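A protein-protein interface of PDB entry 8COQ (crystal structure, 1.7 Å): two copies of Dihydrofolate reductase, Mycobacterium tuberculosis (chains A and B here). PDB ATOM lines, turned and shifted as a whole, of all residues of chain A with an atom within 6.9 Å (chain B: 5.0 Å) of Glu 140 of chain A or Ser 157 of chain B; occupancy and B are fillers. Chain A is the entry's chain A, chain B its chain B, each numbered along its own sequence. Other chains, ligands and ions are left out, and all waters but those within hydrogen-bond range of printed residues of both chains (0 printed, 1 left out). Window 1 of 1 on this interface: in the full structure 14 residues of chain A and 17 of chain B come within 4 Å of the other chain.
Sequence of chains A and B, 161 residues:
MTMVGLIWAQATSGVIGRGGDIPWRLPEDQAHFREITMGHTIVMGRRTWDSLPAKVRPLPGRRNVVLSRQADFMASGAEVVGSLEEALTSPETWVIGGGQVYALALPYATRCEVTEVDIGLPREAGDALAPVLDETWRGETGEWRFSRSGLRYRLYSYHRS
The side-chain carboxylate of Glu 140 of chain A sits at hydrogen-bond distance from the side-chain hydroxyl of Ser 157 of chain B, 3.0 Å away.
O of Leu 155 of chain B lies close to OE2 of Glu 140 of chain A (3.1 Å).
The backbone carbonyl oxygen of Glu 140 of chain A is in hydrogen-bond range of the backbone NH of Ser 157 of chain A (2.9 Å).
O of Leu 155 of chain A is in hydrogen-bond range of N of Gly 142 of chain A (3.0 Å).
OG of Ser 157 of chain B sits at hydrogen-bond distance from OE1 of Glu 113 of chain B.
The backbone NH (N) of Glu 140 of chain B is in hydrogen-bond range of the backbone carbonyl oxygen (O) of Ser 157 of chain B, 3.2 Å away.
N of Gly 142 of chain B is in hydrogen-bond range of O of Leu 155 of chain B, at 2.8 Å.
Gly 139 of chain A touches Arg 145 of chain B (O to NH2, 3.7 Å).
OE2 of Glu 140 of chain A touches CA of Gly 142 of chain B, 3.7 Å away.
CA of Glu 140 of chain A touches NH2 of Arg 145 of chain B, at 3.2 Å.
O of Thr 141 of chain A touches CA of Gly 142 of chain B, at 3.7 Å.
Arg 145 of chain B touches Thr 141 of chain A.
Leu 155 of chain A touches Glu 140 of chain B.
Of the printed residues of chain B, Glu 140 of chain A touches Gly 142, Arg 145, Leu 155 and Ser 157.
Printed residues of chain A within 4 Å of Ser 157 of chain B: Glu 140.
Of the printed residues of chain B, Gly 139 of chain A touches Arg 145 (3.7 Å).
Printed residues of chain A within 4 Å of Arg 145 of chain B: Gly 139, Glu 140 and Thr 141.
Of the printed residues of chain B, Thr 141 of chain A touches Gly 142 (3.7 Å) and Arg 145 (3.6 Å).
Printed residues of chain A within 4 Å of Leu 155 of chain B: Glu 140.
Of the printed residues of chain A, Gly 142 of chain B touches Glu 140 (3.7 Å) and Thr 141 (3.7 Å).
Of the 13 printed residues of chain B, 5 touch a printed residue of chain A.
Hydrophobic or aromatic side chains of chain B within 4 Å of the printed part of chain A: Leu 155.
Of the 12 printed residues of chain A, 4 touch a printed residue of chain B.
Among the printed residues, 8 pairs touch across the chains.
Glu 140 of chain A touches Gly 142 of chain B, but with the chains exchanged Gly 142 of chain A does not touch Glu 140 of chain B (7.0 Å).
Glu 140 of chain A touches Leu 155 of chain B, and with the chains exchanged Leu 155 of chain A touches Glu 140 of chain B.
Glu 140 of chain A touches Ser 157 of chain B, but with the chains exchanged Ser 157 of chain A does not touch Glu 140 of chain B (7.2 Å).
Thr 141 of chain A touches Gly 142 of chain B, but with the chains exchanged Gly 142 of chain A does not touch Thr 141 of chain B (4.05 Å).
11 positions are printed for both chains.
Of the 8 pairs that touch across the chains among the printed residues, 2 have their exchanged pair printed and touching as well.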
ATOM      1  N   ARG A 111      29.191 -28.573   6.670  1.00  0.00           N
ATOM      2  CA  ARG A 111      28.376 -27.609   5.955  1.00  0.00           C
ATOM      3  C   ARG A 111      27.125 -27.326   6.760  1.00  0.00           C
ATOM      4  O   ARG A 111      26.539 -28.240   7.339  1.00  0.00           O
ATOM      5  CB  ARG A 111      27.969 -28.116   4.568  1.00  0.00           C
ATOM      6  CG  ARG A 111      29.102 -28.179   3.581  1.00  0.00           C
ATOM      7  CD  ARG A 111      28.575 -28.628   2.212  1.00  0.00           C
ATOM      8  NE  ARG A 111      27.706 -27.613   1.599  1.00  0.00           N
ATOM      9  CZ  ARG A 111      26.937 -27.846   0.532  1.00  0.00           C
ATOM     10  NH1 ARG A 111      26.956 -29.042  -0.045  1.00  0.00           N
ATOM     11  NH2 ARG A 111      26.173 -26.887   0.024  1.00  0.00           N
ATOM     12  N   GLU A 113      23.653 -25.137   5.727  1.00  0.00           N
ATOM     13  CA  GLU A 113      22.891 -24.336   4.782  1.00  0.00           C
ATOM     14  C   GLU A 113      21.732 -23.713   5.549  1.00  0.00           C
ATOM     15  O   GLU A 113      20.810 -24.417   5.963  1.00  0.00           O
ATOM     16  CB  GLU A 113      22.393 -25.190   3.618  1.00  0.00           C
ATOM     17  CG  GLU A 113      23.519 -25.712   2.728  1.00  0.00           C
ATOM     18  CD  GLU A 113      24.172 -24.597   1.922  1.00  0.00           C
ATOM     19  OE1 GLU A 113      23.475 -23.613   1.589  1.00  0.00           O
ATOM     20  OE2 GLU A 113      25.377 -24.713   1.610  1.00  0.00           O
ATOM     21  N   ARG A 138      33.157 -20.796   8.627  1.00  0.00           N
ATOM     22  CA  ARG A 138      33.287 -19.749   7.622  1.00  0.00           C
ATOM     23  C   ARG A 138      31.986 -19.674   6.831  1.00  0.00           C
ATOM     24  O   ARG A 138      31.536 -20.679   6.268  1.00  0.00           O
ATOM     25  CB  ARG A 138      34.470 -20.047   6.704  1.00  0.00           C
ATOM     26  CG  ARG A 138      34.597 -19.138   5.485  1.00  0.00           C
ATOM     27  CD  ARG A 138      35.858 -19.497   4.700  1.00  0.00           C
ATOM     28  NE  ARG A 138      37.031 -18.767   5.163  1.00  0.00           N
ATOM     29  CZ  ARG A 138      37.619 -17.809   4.455  1.00  0.00           C
ATOM     30  NH1 ARG A 138      37.139 -17.498   3.257  1.00  0.00           N
ATOM     31  NH2 ARG A 138      38.685 -17.177   4.934  1.00  0.00           N
ATOM     32  N   GLY A 139      31.372 -18.500   6.808  1.00  0.00           N
ATOM     33  CA  GLY A 139      30.066 -18.383   6.188  1.00  0.00           C
ATOM     34  C   GLY A 139      30.027 -17.454   4.997  1.00  0.00           C
ATOM     35  O   GLY A 139      30.583 -16.352   5.046  1.00  0.00           O
ATOM     36  N   GLU A 140      29.500 -17.746   3.512  1.00  0.00           N
ATOM     37  CA  GLU A 140      28.908 -17.042   2.380  1.00  0.00           C
ATOM     38  C   GLU A 140      27.548 -16.500   2.798  1.00  0.00           C
ATOM     39  O   GLU A 140      26.657 -17.271   3.170  1.00  0.00           O
ATOM     40  CB  GLU A 140      28.775 -17.963   1.166  1.00  0.00           C
ATOM     41  CG  GLU A 140      28.231 -17.278  -0.078  1.00  0.00           C
ATOM     42  CD  GLU A 140      28.160 -18.211  -1.271  1.00  0.00           C
ATOM     43  OE1 GLU A 140      28.501 -19.402  -1.117  1.00  0.00           O
ATOM     44  OE2 GLU A 140      27.766 -17.752  -2.364  1.00  0.00           O
ATOM     45  N   THR A 141      27.426 -15.360   2.727  1.00  0.00           N
ATOM     46  CA  THR A 141      26.094 -14.782   2.806  1.00  0.00           C
ATOM     47  C   THR A 141      25.586 -14.411   1.414  1.00  0.00           C
ATOM     48  O   THR A 141      26.361 -13.970   0.559  1.00  0.00           O
ATOM     49  CB  THR A 141      26.126 -13.533   3.694  1.00  0.00           C
ATOM     50  OG1 THR A 141      26.693 -13.856   4.973  1.00  0.00           O
ATOM     51  CG2 THR A 141      24.741 -12.963   3.886  1.00  0.00           C
ATOM     52  N   GLY A 142      24.281 -14.593   1.189  1.00  0.00           N
ATOM     53  CA  GLY A 142      23.603 -14.017   0.048  1.00  0.00           C
ATOM     54  C   GLY A 142      22.789 -12.782   0.430  1.00  0.00           C
ATOM     55  O   GLY A 142      22.743 -12.355   1.581  1.00  0.00           O
ATOM     56  N   LEU A 155      19.940 -16.616   2.298  1.00  0.00           N
ATOM     57  CA  LEU A 155      20.567 -17.919   2.450  1.00  0.00           C
ATOM     58  C   LEU A 155      22.011 -17.729   2.893  1.00  0.00           C
ATOM     59  O   LEU A 155      22.743 -16.929   2.299  1.00  0.00           O
ATOM     60  CB  LEU A 155      20.498 -18.712   1.150  1.00  0.00           C
ATOM     61  CG  LEU A 155      19.084 -18.743   0.555  1.00  0.00           C
ATOM     62  CD1 LEU A 155      19.035 -19.542  -0.749  1.00  0.00           C
ATOM     63  CD2 LEU A 155      18.029 -19.220   1.548  1.00  0.00           C
ATOM     64  N   TYR A 156      22.397 -18.432   3.958  1.00  0.00           N
ATOM     65  CA  TYR A 156      23.784 -18.530   4.409  1.00  0.00           C
ATOM     66  C   TYR A 156      24.319 -19.910   4.070  1.00  0.00           C
ATOM     67  O   TYR A 156      23.662 -20.917   4.359  1.00  0.00           O
ATOM     68  CB  TYR A 156      23.909 -18.361   5.925  1.00  0.00           C
ATOM     69  CG  TYR A 156      23.594 -17.016   6.490  1.00  0.00           C
ATOM     70  CD1 TYR A 156      22.279 -16.625   6.693  1.00  0.00           C
ATOM     71  CD2 TYR A 156      24.605 -16.158   6.887  1.00  0.00           C
ATOM     72  CE1 TYR A 156      21.977 -15.399   7.238  1.00  0.00           C
ATOM     73  CE2 TYR A 156      24.315 -14.923   7.432  1.00  0.00           C
ATOM     74  CZ  TYR A 156      22.995 -14.546   7.608  1.00  0.00           C
ATOM     75  OH  TYR A 156      22.680 -13.319   8.156  1.00  0.00           O
ATOM     76  N   SER A 157      25.526 -19.969   3.516  1.00  0.00           N
ATOM     77  CA  SER A 157      26.216 -21.238   3.321  1.00  0.00           C
ATOM     78  C   SER A 157      27.476 -21.221   4.191  1.00  0.00           C
ATOM     79  O   SER A 157      28.426 -20.494   3.893  1.00  0.00           O
ATOM     80  CB  SER A 157      26.542 -21.458   1.842  1.00  0.00           C
ATOM     81  OG  SER A 157      27.154 -22.715   1.632  1.00  0.00           O
ATOM     82  N   TYR A 158      27.475 -21.990   5.282  1.00  0.00           N
ATOM     83  CA  TYR A 158      28.632 -22.082   6.169  1.00  0.00           C
ATOM     84  C   TYR A 158      29.435 -23.338   5.877  1.00  0.00           C
ATOM     85  O   TYR A 158      28.879 -24.391   5.553  1.00  0.00           O
ATOM     86  CB  TYR A 158      28.229 -22.095   7.648  1.00  0.00           C
ATOM     87  CG  TYR A 158      27.576 -20.852   8.194  1.00  0.00           C
ATOM     88  CD1 TYR A 158      26.192 -20.677   8.130  1.00  0.00           C
ATOM     89  CD2 TYR A 158      28.328 -19.885   8.852  1.00  0.00           C
ATOM     90  CE1 TYR A 158      25.597 -19.562   8.661  1.00  0.00           C
ATOM     91  CE2 TYR A 158      27.733 -18.757   9.382  1.00  0.00           C
ATOM     92  CZ  TYR A 158      26.364 -18.607   9.285  1.00  0.00           C
ATOM     93  OH  TYR A 158      25.759 -17.489   9.812  1.00  0.00           O
ATOM     94  N   HIS A 159      30.753 -23.230   6.015  1.00  0.00           N
ATOM     95  CA  HIS A 159      31.622 -24.368   5.806  1.00  0.00           C
ATOM     96  C   HIS A 159      32.797 -24.274   6.757  1.00  0.00           C
ATOM     97  O   HIS A 159      33.229 -23.186   7.146  1.00  0.00           O
ATOM     98  CB  HIS A 159      32.082 -24.486   4.328  1.00  0.00           C
ATOM     99  CG  HIS A 159      33.130 -25.537   4.076  1.00  0.00           C
ATOM    100  ND1 HIS A 159      34.419 -25.454   4.570  1.00  0.00           N
ATOM    101  CD2 HIS A 159      33.054 -26.734   3.438  1.00  0.00           C
ATOM    102  CE1 HIS A 159      35.102 -26.527   4.204  1.00  0.00           C
ATOM    103  NE2 HIS A 159      34.295 -27.324   3.525  1.00  0.00           N
ATOM    104  N   CYS B 112      29.430 -26.964  -8.418  1.00  0.00           N
ATOM    105  CA  CYS B 112      30.479 -26.035  -8.845  1.00  0.00           C
ATOM    106  C   CYS B 112      30.530 -24.858  -7.886  1.00  0.00           C
ATOM    107  O   CYS B 112      29.514 -24.187  -7.666  1.00  0.00           O
ATOM    108  CB  CYS B 112      30.257 -25.503 -10.269  1.00  0.00           C
ATOM    109  SG  CYS B 112      30.324 -26.724 -11.580  1.00  0.00           S
ATOM    110  N   GLU B 113      31.715 -24.590  -7.325  1.00  0.00           N
ATOM    111  CA  GLU B 113      31.949 -23.430  -6.468  1.00  0.00           C
ATOM    112  C   GLU B 113      32.751 -22.414  -7.283  1.00  0.00           C
ATOM    113  O   GLU B 113      33.924 -22.654  -7.611  1.00  0.00           O
ATOM    114  CB  GLU B 113      32.675 -23.861  -5.195  1.00  0.00           C
ATOM    115  CG  GLU B 113      31.820 -24.813  -4.346  1.00  0.00           C
ATOM    116  CD  GLU B 113      30.630 -24.120  -3.696  1.00  0.00           C
ATOM    117  OE1 GLU B 113      30.644 -22.867  -3.611  1.00  0.00           O
ATOM    118  OE2 GLU B 113      29.667 -24.819  -3.295  1.00  0.00           O
ATOM    119  N   ARG B 138      21.440 -25.202 -10.831  1.00  0.00           N
ATOM    120  CA  ARG B 138      20.782 -24.200 -10.010  1.00  0.00           C
ATOM    121  C   ARG B 138      21.850 -23.564  -9.133  1.00  0.00           C
ATOM    122  O   ARG B 138      22.648 -24.271  -8.510  1.00  0.00           O
ATOM    123  CB  ARG B 138      19.674 -24.828  -9.160  1.00  0.00           C
ATOM    124  CG  ARG B 138      18.842 -25.888  -9.893  1.00  0.00           C
ATOM    125  CD  ARG B 138      17.774 -25.328 -10.836  1.00  0.00           C
ATOM    126  NE  ARG B 138      16.749 -26.335 -11.126  1.00  0.00           N
ATOM    127  CZ  ARG B 138      16.200 -26.538 -12.323  1.00  0.00           C
ATOM    128  NH1 ARG B 138      16.583 -25.817 -13.370  1.00  0.00           N
ATOM    129  NH2 ARG B 138      15.275 -27.480 -12.480  1.00  0.00           N
ATOM    130  N   GLY B 139      21.887 -22.242  -9.093  1.00  0.00           N
ATOM    131  CA  GLY B 139      22.938 -21.545  -8.383  1.00  0.00           C
ATOM    132  C   GLY B 139      22.417 -20.464  -7.462  1.00  0.00           C
ATOM    133  O   GLY B 139      21.379 -19.852  -7.704  1.00  0.00           O
ATOM    134  N   GLU B 140      23.167 -20.235  -6.393  1.00  0.00           N
ATOM    135  CA  GLU B 140      22.879 -19.165  -5.451  1.00  0.00           C
ATOM    136  C   GLU B 140      23.964 -18.111  -5.584  1.00  0.00           C
ATOM    137  O   GLU B 140      25.143 -18.392  -5.331  1.00  0.00           O
ATOM    138  CB  GLU B 140      22.795 -19.684  -4.014  1.00  0.00           C
ATOM    139  CG  GLU B 140      21.512 -20.466  -3.664  1.00  0.00           C
ATOM    140  CD  GLU B 140      20.209 -19.845  -4.189  1.00  0.00           C
ATOM    141  OE1 GLU B 140      20.145 -18.616  -4.436  1.00  0.00           O
ATOM    142  OE2 GLU B 140      19.234 -20.610  -4.359  1.00  0.00           O
ATOM    143  N   THR B 141      23.563 -16.914  -6.004  1.00  0.00           N
ATOM    144  CA  THR B 141      24.482 -15.790  -6.061  1.00  0.00           C
ATOM    145  C   THR B 141      24.775 -15.284  -4.657  1.00  0.00           C
ATOM    146  O   THR B 141      23.860 -15.025  -3.866  1.00  0.00           O
ATOM    147  CB  THR B 141      23.890 -14.663  -6.903  1.00  0.00           C
ATOM    148  OG1 THR B 141      23.598 -15.143  -8.221  1.00  0.00           O
ATOM    149  CG2 THR B 141      24.857 -13.500  -6.989  1.00  0.00           C
ATOM    150  N   GLY B 142      26.049 -15.159  -4.341  1.00  0.00           N
ATOM    151  CA  GLY B 142      26.426 -14.433  -3.157  1.00  0.00           C
ATOM    152  C   GLY B 142      26.447 -12.933  -3.398  1.00  0.00           C
ATOM    153  O   GLY B 142      26.430 -12.436  -4.526  1.00  0.00           O
ATOM    154  N   ARG B 145      31.396  -9.225  -2.498  1.00  0.00           N
ATOM    155  CA  ARG B 145      32.358  -8.861  -1.466  1.00  0.00           C
ATOM    156  C   ARG B 145      33.382  -7.884  -2.044  1.00  0.00           C
ATOM    157  O   ARG B 145      33.384  -7.582  -3.241  1.00  0.00           O
ATOM    158  CB  ARG B 145      33.123 -10.058  -0.900  1.00  0.00           C
ATOM    159  CG  ARG B 145      32.567 -10.957   0.204  1.00  0.00           C
ATOM    160  CD  ARG B 145      31.633 -12.024  -0.252  1.00  0.00           C
ATOM    161  NE  ARG B 145      31.891 -13.177   0.621  1.00  0.00           N
ATOM    162  CZ  ARG B 145      31.050 -14.183   0.791  1.00  0.00           C
ATOM    163  NH1 ARG B 145      29.909 -14.166   0.123  1.00  0.00           N
ATOM    164  NH2 ARG B 145      31.361 -15.210   1.579  1.00  0.00           N
ATOM    165  N   LEU B 155      30.725 -14.835  -5.031  1.00  0.00           N
ATOM    166  CA  LEU B 155      30.789 -16.288  -4.937  1.00  0.00           C
ATOM    167  C   LEU B 155      29.477 -16.894  -5.417  1.00  0.00           C
ATOM    168  O   LEU B 155      28.400 -16.415  -5.048  1.00  0.00           O
ATOM    169  CB  LEU B 155      31.068 -16.718  -3.498  1.00  0.00           C
ATOM    170  CG  LEU B 155      32.433 -16.273  -2.971  1.00  0.00           C
ATOM    171  CD1 LEU B 155      32.662 -16.775  -1.551  1.00  0.00           C
ATOM    172  CD2 LEU B 155      33.527 -16.731  -3.899  1.00  0.00           C
ATOM    173  N   TYR B 156      29.567 -17.933  -6.252  1.00  0.00           N
ATOM    174  CA  TYR B 156      28.415 -18.725  -6.667  1.00  0.00           C
ATOM    175  C   TYR B 156      28.564 -20.157  -6.172  1.00  0.00           C
ATOM    176  O   TYR B 156      29.622 -20.768  -6.342  1.00  0.00           O
ATOM    177  CB  TYR B 156      28.252 -18.765  -8.184  1.00  0.00           C
ATOM    178  CG  TYR B 156      28.025 -17.436  -8.848  1.00  0.00           C
ATOM    179  CD1 TYR B 156      29.047 -16.503  -8.954  1.00  0.00           C
ATOM    180  CD2 TYR B 156      26.778 -17.111  -9.372  1.00  0.00           C
ATOM    181  CE1 TYR B 156      28.838 -15.285  -9.577  1.00  0.00           C
ATOM    182  CE2 TYR B 156      26.556 -15.903  -9.983  1.00  0.00           C
ATOM    183  CZ  TYR B 156      27.585 -14.992 -10.087  1.00  0.00           C
ATOM    184  OH  TYR B 156      27.354 -13.783 -10.703  1.00  0.00           O
ATOM    185  N   SER B 157      27.501 -20.702  -5.590  1.00  0.00           N
ATOM    186  CA  SER B 157      27.437 -22.124  -5.254  1.00  0.00           C
ATOM    187  C   SER B 157      26.403 -22.778  -6.170  1.00  0.00           C
ATOM    188  O   SER B 157      25.194 -22.663  -5.939  1.00  0.00           O
ATOM    189  CB  SER B 157      27.093 -22.337  -3.782  1.00  0.00           C
ATOM    190  OG  SER B 157      28.068 -21.760  -2.930  1.00  0.00           O
ATOM    191  N   TYR B 158      26.875 -23.464  -7.208  1.00  0.00           N
ATOM    192  CA  TYR B 158      26.003 -24.192  -8.114  1.00  0.00           C
ATOM    193  C   TYR B 158      25.871 -25.653  -7.715  1.00  0.00           C
ATOM    194  O   TYR B 158      26.832 -26.300  -7.287  1.00  0.00           O
ATOM    195  CB  TYR B 158      26.513 -24.130  -9.551  1.00  0.00           C
ATOM    196  CG  TYR B 158      26.474 -22.771 -10.196  1.00  0.00           C
ATOM    197  CD1 TYR B 158      25.302 -22.287 -10.753  1.00  0.00           C
ATOM    198  CD2 TYR B 158      27.615 -21.987 -10.280  1.00  0.00           C
ATOM    199  CE1 TYR B 158      25.265 -21.049 -11.357  1.00  0.00           C
ATOM    200  CE2 TYR B 158      27.590 -20.754 -10.877  1.00  0.00           C
ATOM    201  CZ  TYR B 158      26.411 -20.290 -11.415  1.00  0.00           C
ATOM    202  OH  TYR B 158      26.387 -19.059 -12.016  1.00  0.00           O
ATOM    203  N   HIS B 159      24.667 -26.176  -7.921  1.00  0.00           N
ATOM    204  CA  HIS B 159      24.279 -27.539  -7.601  1.00  0.00           C
ATOM    205  C   HIS B 159      23.337 -28.080  -8.659  1.00  0.00           C
ATOM    206  O   HIS B 159      22.555 -27.330  -9.247  1.00  0.00           O
ATOM    207  CB  HIS B 159      23.600 -27.600  -6.236  1.00  0.00           C
ATOM    208  CG  HIS B 159      23.172 -28.972  -5.849  1.00  0.00           C
ATOM    209  ND1 HIS B 159      21.935 -29.472  -6.206  1.00  0.00           N
ATOM    210  CD2 HIS B 159      23.798 -29.958  -5.163  1.00  0.00           C
ATOM    211  CE1 HIS B 159      21.818 -30.703  -5.744  1.00  0.00           C
ATOM    212  NE2 HIS B 159      22.932 -31.021  -5.107  1.00  0.00           N
